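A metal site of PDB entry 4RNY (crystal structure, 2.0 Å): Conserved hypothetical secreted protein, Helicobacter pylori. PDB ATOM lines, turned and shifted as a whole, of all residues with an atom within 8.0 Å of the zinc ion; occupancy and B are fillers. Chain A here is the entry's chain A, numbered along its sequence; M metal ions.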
ATOM      1  N   SER A  30      19.154  11.430   4.402  1.00  0.00           N
ATOM      2  CA  SER A  30      19.144   9.991   4.075  1.00  0.00           C
ATOM      3  C   SER A  30      19.324   9.078   5.308  1.00  0.00           C
ATOM      4  O   SER A  30      18.714   8.007   5.369  1.00  0.00           O
ATOM      5  CB  SER A  30      20.214   9.672   3.044  1.00  0.00           C
ATOM      6  OG  SER A  30      21.387  10.337   3.409  1.00  0.00           O
ATOM      7  N   GLN A  31      20.076   9.518   6.296  1.00  0.00           N
ATOM      8  CA  GLN A  31      20.235   8.739   7.536  1.00  0.00           C
ATOM      9  C   GLN A  31      18.886   8.603   8.266  1.00  0.00           C
ATOM     10  O   GLN A  31      18.495   7.503   8.645  1.00  0.00           O
ATOM     11  CB  GLN A  31      21.307   9.346   8.486  1.00  0.00           C
ATOM     12  CG  GLN A  31      22.691   9.504   7.876  1.00  0.00           C
ATOM     13  CD  GLN A  31      22.893  10.820   7.088  1.00  0.00           C
ATOM     14  OE1 GLN A  31      21.931  11.452   6.636  1.00  0.00           O
ATOM     15  NE2 GLN A  31      24.153  11.201   6.886  1.00  0.00           N
ATOM     16  N   GLU A  34      16.675   6.196   6.434  1.00  0.00           N
ATOM     17  CA  GLU A  34      17.009   4.824   6.818  1.00  0.00           C
ATOM     18  C   GLU A  34      16.328   4.454   8.123  1.00  0.00           C
ATOM     19  O   GLU A  34      15.795   3.369   8.237  1.00  0.00           O
ATOM     20  CB  GLU A  34      18.522   4.623   7.013  1.00  0.00           C
ATOM     21  CG  GLU A  34      19.330   4.564   5.753  1.00  0.00           C
ATOM     22  CD  GLU A  34      20.709   3.986   5.981  1.00  0.00           C
ATOM     23  OE1 GLU A  34      21.237   3.448   4.999  1.00  0.00           O
ATOM     24  OE2 GLU A  34      21.270   4.097   7.126  1.00  0.00           O
ATOM     25  N   LEU A  35      16.355   5.355   9.107  1.00  0.00           N
ATOM     26  CA  LEU A  35      15.703   5.066  10.419  1.00  0.00           C
ATOM     27  C   LEU A  35      14.223   4.836  10.197  1.00  0.00           C
ATOM     28  O   LEU A  35      13.619   3.923  10.751  1.00  0.00           O
ATOM     29  CB  LEU A  35      15.898   6.227  11.374  1.00  0.00           C
ATOM     30  CG  LEU A  35      17.275   6.419  11.967  1.00  0.00           C
ATOM     31  CD1 LEU A  35      17.331   7.699  12.767  1.00  0.00           C
ATOM     32  CD2 LEU A  35      17.582   5.242  12.888  1.00  0.00           C
ATOM     33  N   SER A 201      31.681   3.681   6.398  1.00  0.00           N
ATOM     34  CA  SER A 201      31.333   5.082   6.283  1.00  0.00           C
ATOM     35  C   SER A 201      30.465   5.515   7.420  1.00  0.00           C
ATOM     36  O   SER A 201      30.511   6.652   7.793  1.00  0.00           O
ATOM     37  CB  SER A 201      30.643   5.381   4.954  1.00  0.00           C
ATOM     38  OG  SER A 201      29.372   4.776   4.861  1.00  0.00           O
ATOM     39  N   SER A 202      29.667   4.617   7.990  1.00  0.00           N
ATOM     40  CA  SER A 202      28.982   4.916   9.229  1.00  0.00           C
ATOM     41  C   SER A 202      28.789   3.644  10.054  1.00  0.00           C
ATOM     42  O   SER A 202      28.120   2.679   9.626  1.00  0.00           O
ATOM     43  CB  SER A 202      27.653   5.637   8.930  1.00  0.00           C
ATOM     44  OG  SER A 202      26.936   5.939  10.136  1.00  0.00           O
ATOM     45  N   PRO A 203      29.364   3.624  11.247  1.00  0.00           N
ATOM     46  CA  PRO A 203      29.225   2.442  12.022  1.00  0.00           C
ATOM     47  C   PRO A 203      27.870   2.334  12.655  1.00  0.00           C
ATOM     48  O   PRO A 203      27.070   3.267  12.579  1.00  0.00           O
ATOM     49  CB  PRO A 203      30.324   2.617  13.094  1.00  0.00           C
ATOM     50  CG  PRO A 203      30.410   4.065  13.279  1.00  0.00           C
ATOM     51  CD  PRO A 203      30.259   4.600  11.884  1.00  0.00           C
ATOM     52  N   PHE A 204      27.609   1.194  13.278  1.00  0.00           N
ATOM     53  CA  PHE A 204      26.394   1.023  14.086  1.00  0.00           C
ATOM     54  C   PHE A 204      26.462   1.970  15.286  1.00  0.00           C
ATOM     55  O   PHE A 204      27.543   2.169  15.814  1.00  0.00           O
ATOM     56  CB  PHE A 204      26.298  -0.422  14.568  1.00  0.00           C
ATOM     57  CG  PHE A 204      25.053  -0.737  15.412  1.00  0.00           C
ATOM     58  CD1 PHE A 204      25.037  -0.521  16.803  1.00  0.00           C
ATOM     59  CD2 PHE A 204      23.912  -1.242  14.816  1.00  0.00           C
ATOM     60  CE1 PHE A 204      23.894  -0.755  17.531  1.00  0.00           C
ATOM     61  CE2 PHE A 204      22.782  -1.545  15.551  1.00  0.00           C
ATOM     62  CZ  PHE A 204      22.770  -1.284  16.928  1.00  0.00           C
ATOM     63  N   HIS A 219      22.216   4.718  14.671  1.00  0.00           N
ATOM     64  CA  HIS A 219      22.226   4.136  13.315  1.00  0.00           C
ATOM     65  C   HIS A 219      22.184   2.612  13.460  1.00  0.00           C
ATOM     66  O   HIS A 219      23.104   1.999  13.997  1.00  0.00           O
ATOM     67  CB  HIS A 219      23.487   4.601  12.586  1.00  0.00           C
ATOM     68  CG  HIS A 219      23.694   3.972  11.249  1.00  0.00           C
ATOM     69  ND1 HIS A 219      24.905   3.473  10.842  1.00  0.00           N
ATOM     70  CD2 HIS A 219      22.861   3.808  10.200  1.00  0.00           C
ATOM     71  CE1 HIS A 219      24.814   3.035   9.606  1.00  0.00           C
ATOM     72  NE2 HIS A 219      23.583   3.205   9.205  1.00  0.00           N
ATOM     73  N   TYR A 220      21.138   1.970  12.944  1.00  0.00           N
ATOM     74  CA  TYR A 220      20.901   0.581  13.303  1.00  0.00           C
ATOM     75  C   TYR A 220      21.430  -0.442  12.315  1.00  0.00           C
ATOM     76  O   TYR A 220      20.895  -1.547  12.176  1.00  0.00           O
ATOM     77  CB  TYR A 220      19.444   0.363  13.556  1.00  0.00           C
ATOM     78  CG  TYR A 220      18.921   1.136  14.752  1.00  0.00           C
ATOM     79  CD1 TYR A 220      19.479   0.974  15.999  1.00  0.00           C
ATOM     80  CD2 TYR A 220      17.799   1.957  14.619  1.00  0.00           C
ATOM     81  CE1 TYR A 220      18.939   1.636  17.118  1.00  0.00           C
ATOM     82  CE2 TYR A 220      17.264   2.627  15.717  1.00  0.00           C
ATOM     83  CZ  TYR A 220      17.853   2.458  16.976  1.00  0.00           C
ATOM     84  OH  TYR A 220      17.294   3.142  18.062  1.00  0.00           O
ATOM     85  N   GLY A 221      22.528  -0.076  11.701  1.00  0.00           N
ATOM     86  CA  GLY A 221      23.292  -1.003  10.871  1.00  0.00           C
ATOM     87  C   GLY A 221      24.639  -0.408  10.612  1.00  0.00           C
ATOM     88  O   GLY A 221      25.022   0.520  11.329  1.00  0.00           O
ATOM     89  N   VAL A 222      25.359  -0.986   9.652  1.00  0.00           N
ATOM     90  CA  VAL A 222      26.680  -0.534   9.240  1.00  0.00           C
ATOM     91  C   VAL A 222      26.613  -0.089   7.799  1.00  0.00           C
ATOM     92  O   VAL A 222      26.106  -0.817   6.936  1.00  0.00           O
ATOM     93  CB  VAL A 222      27.729  -1.689   9.252  1.00  0.00           C
ATOM     94  CG1 VAL A 222      29.138  -1.133   8.972  1.00  0.00           C
ATOM     95  CG2 VAL A 222      27.712  -2.440  10.537  1.00  0.00           C
ATOM     96  N   ASP A 223      27.105   1.110   7.516  1.00  0.00           N
ATOM     97  CA  ASP A 223      27.135   1.586   6.142  1.00  0.00           C
ATOM     98  C   ASP A 223      28.558   1.341   5.623  1.00  0.00           C
ATOM     99  O   ASP A 223      29.516   1.821   6.184  1.00  0.00           O
ATOM    100  CB  ASP A 223      26.801   3.080   6.080  1.00  0.00           C
ATOM    101  CG  ASP A 223      25.316   3.355   6.254  1.00  0.00           C
ATOM    102  OD1 ASP A 223      24.512   2.420   6.341  1.00  0.00           O
ATOM    103  OD2 ASP A 223      24.952   4.538   6.357  1.00  0.00           O
ATOM    104  N   TYR A 224      28.664   0.585   4.548  1.00  0.00           N
ATOM    105  CA  TYR A 224      29.961   0.291   3.916  1.00  0.00           C
ATOM    106  C   TYR A 224      30.125   1.150   2.645  1.00  0.00           C
ATOM    107  O   TYR A 224      29.225   1.164   1.798  1.00  0.00           O
ATOM    108  CB  TYR A 224      29.990  -1.170   3.472  1.00  0.00           C
ATOM    109  CG  TYR A 224      30.031  -2.222   4.570  1.00  0.00           C
ATOM    110  CD1 TYR A 224      31.202  -2.506   5.237  1.00  0.00           C
ATOM    111  CD2 TYR A 224      28.897  -2.947   4.904  1.00  0.00           C
ATOM    112  CE1 TYR A 224      31.251  -3.471   6.201  1.00  0.00           C
ATOM    113  CE2 TYR A 224      28.938  -3.933   5.877  1.00  0.00           C
ATOM    114  CZ  TYR A 224      30.112  -4.189   6.537  1.00  0.00           C
ATOM    115  OH  TYR A 224      30.217  -5.179   7.505  1.00  0.00           O
ATOM    116  N   GLY A 248      13.596   4.813   1.853  1.00  0.00           N
ATOM    117  CA  GLY A 248      14.685   4.982   2.801  1.00  0.00           C
ATOM    118  C   GLY A 248      15.796   3.965   2.707  1.00  0.00           C
ATOM    119  O   GLY A 248      16.909   4.207   3.246  1.00  0.00           O
ATOM    120  N   TYR A 249      15.479   2.807   2.103  1.00  0.00           N
ATOM    121  CA  TYR A 249      16.447   1.721   1.844  1.00  0.00           C
ATOM    122  C   TYR A 249      16.689   1.431   0.346  1.00  0.00           C
ATOM    123  O   TYR A 249      17.588   0.636   0.006  1.00  0.00           O
ATOM    124  CB  TYR A 249      15.949   0.407   2.432  1.00  0.00           C
ATOM    125  CG  TYR A 249      16.169   0.117   3.914  1.00  0.00           C
ATOM    126  CD1 TYR A 249      17.166   0.743   4.646  1.00  0.00           C
ATOM    127  CD2 TYR A 249      15.441  -0.904   4.541  1.00  0.00           C
ATOM    128  CE1 TYR A 249      17.376   0.427   5.991  1.00  0.00           C
ATOM    129  CE2 TYR A 249      15.636  -1.216   5.880  1.00  0.00           C
ATOM    130  CZ  TYR A 249      16.628  -0.536   6.591  1.00  0.00           C
ATOM    131  OH  TYR A 249      16.881  -0.812   7.901  1.00  0.00           O
ATOM    132  N   ALA A 265      20.683  -3.186   2.160  1.00  0.00           N
ATOM    133  CA  ALA A 265      19.940  -2.107   1.554  1.00  0.00           C
ATOM    134  C   ALA A 265      20.792  -1.186   0.642  1.00  0.00           C
ATOM    135  O   ALA A 265      22.034  -1.108   0.759  1.00  0.00           O
ATOM    136  CB  ALA A 265      19.266  -1.294   2.656  1.00  0.00           C
ATOM    137  N   HIS A 266      20.084  -0.475  -0.220  1.00  0.00           N
ATOM    138  CA  HIS A 266      20.636   0.416  -1.243  1.00  0.00           C
ATOM    139  C   HIS A 266      21.289  -0.342  -2.405  1.00  0.00           C
ATOM    140  O   HIS A 266      22.227   0.148  -3.002  1.00  0.00           O
ATOM    141  CB  HIS A 266      21.625   1.445  -0.651  1.00  0.00           C
ATOM    142  CG  HIS A 266      21.103   2.149   0.564  1.00  0.00           C
ATOM    143  ND1 HIS A 266      19.991   2.957   0.530  1.00  0.00           N
ATOM    144  CD2 HIS A 266      21.537   2.167   1.848  1.00  0.00           C
ATOM    145  CE1 HIS A 266      19.762   3.439   1.734  1.00  0.00           C
ATOM    146  NE2 HIS A 266      20.685   2.974   2.555  1.00  0.00           N
ATOM    147  N   HIS A 299      26.841   2.768  -1.594  1.00  0.00           N
ATOM    148  CA  HIS A 299      26.869   2.249  -0.198  1.00  0.00           C
ATOM    149  C   HIS A 299      25.958   1.054   0.007  1.00  0.00           C
ATOM    150  O   HIS A 299      25.001   0.855  -0.727  1.00  0.00           O
ATOM    151  CB  HIS A 299      26.487   3.344   0.799  1.00  0.00           C
ATOM    152  CG  HIS A 299      27.490   4.459   0.882  1.00  0.00           C
ATOM    153  ND1 HIS A 299      28.597   4.409   1.696  1.00  0.00           N
ATOM    154  CD2 HIS A 299      27.534   5.662   0.268  1.00  0.00           C
ATOM    155  CE1 HIS A 299      29.288   5.529   1.572  1.00  0.00           C
ATOM    156  NE2 HIS A 299      28.666   6.310   0.712  1.00  0.00           N
ATOM    157  N   LEU A 300      26.316   0.205   0.949  1.00  0.00           N
ATOM    158  CA  LEU A 300      25.470  -0.871   1.387  1.00  0.00           C
ATOM    159  C   LEU A 300      25.123  -0.511   2.837  1.00  0.00           C
ATOM    160  O   LEU A 300      26.006  -0.104   3.581  1.00  0.00           O
ATOM    161  CB  LEU A 300      26.206  -2.220   1.337  1.00  0.00           C
ATOM    162  CG  LEU A 300      25.516  -3.358   2.102  1.00  0.00           C
ATOM    163  CD1 LEU A 300      24.277  -3.835   1.368  1.00  0.00           C
ATOM    164  CD2 LEU A 300      26.437  -4.533   2.370  1.00  0.00           C
ATOM    165  N   HIS A 301      23.860  -0.615   3.220  1.00  0.00           N
ATOM    166  CA  HIS A 301      23.520  -0.529   4.645  1.00  0.00           C
ATOM    167  C   HIS A 301      23.263  -1.954   5.034  1.00  0.00           C
ATOM    168  O   HIS A 301      22.424  -2.589   4.429  1.00  0.00           O
ATOM    169  CB  HIS A 301      22.293   0.328   4.875  1.00  0.00           C
ATOM    170  CG  HIS A 301      21.656   0.141   6.211  1.00  0.00           C
ATOM    171  ND1 HIS A 301      21.886   0.995   7.264  1.00  0.00           N
ATOM    172  CD2 HIS A 301      20.804  -0.800   6.682  1.00  0.00           C
ATOM    173  CE1 HIS A 301      21.147   0.625   8.292  1.00  0.00           C
ATOM    174  NE2 HIS A 301      20.499  -0.473   7.972  1.00  0.00           N
ATOM    175  N   PHE A 302      24.042  -2.461   5.954  1.00  0.00           N
ATOM    176  CA  PHE A 302      23.878  -3.832   6.413  1.00  0.00           C
ATOM    177  C   PHE A 302      23.351  -3.796   7.831  1.00  0.00           C
ATOM    178  O   PHE A 302      24.015  -3.252   8.701  1.00  0.00           O
ATOM    179  CB  PHE A 302      25.223  -4.506   6.403  1.00  0.00           C
ATOM    180  CG  PHE A 302      25.248  -5.922   6.935  1.00  0.00           C
ATOM    181  CD1 PHE A 302      24.332  -6.865   6.538  1.00  0.00           C
ATOM    182  CD2 PHE A 302      26.258  -6.314   7.789  1.00  0.00           C
ATOM    183  CE1 PHE A 302      24.405  -8.176   6.961  1.00  0.00           C
ATOM    184  CE2 PHE A 302      26.356  -7.620   8.249  1.00  0.00           C
ATOM    185  CZ  PHE A 302      25.411  -8.557   7.849  1.00  0.00           C
ATOM    186  N   GLY A 303      22.181  -4.389   8.029  1.00  0.00           N
ATOM    187  CA  GLY A 303      21.515  -4.456   9.318  1.00  0.00           C
ATOM    188  C   GLY A 303      21.318  -5.881   9.796  1.00  0.00           C
ATOM    189  O   GLY A 303      20.945  -6.770   8.979  1.00  0.00           O
HETATM  190 ZN    ZN M   1      22.782   2.788   7.306  1.00  0.00          ZN
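The backbone NH of Ser 201 sits at hydrogen-bond distance from the backbone carbonyl oxygen of Asp 223, at 2.9 Å.
A ring nitrogen (ND1) of His 219 sits at hydrogen-bond distance from the backbone carbonyl oxygen (O) of Gly 221, 3.0 Å away.
The side-chain hydroxyl of Ser 202 is in hydrogen-bond range of a ring nitrogen (ND1) of His 219 (3.3 Å).
NE2 of His 266 sits at hydrogen-bond distance from OE1 of Glu 34 (2.6 Å).
A ring nitrogen (ND1) of His 219 is in hydrogen-bond range of the backbone carbonyl oxygen (O) of Pro 203 (2.8 Å).
N of Ala 265 lies within hydrogen-bond range of O of His 301, at 2.9 Å.
The backbone NH of Asp 223 lies within hydrogen-bond range of the backbone carbonyl oxygen of Ser 202 (2.8 Å).
Along chain A the residues within 4 Å of the zinc ion span positions 34 to 301.
The zinc ion is bound by ND1 of His 301, OE2 of Glu 34, OD1 of Asp 223 and NE2 of His 219.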
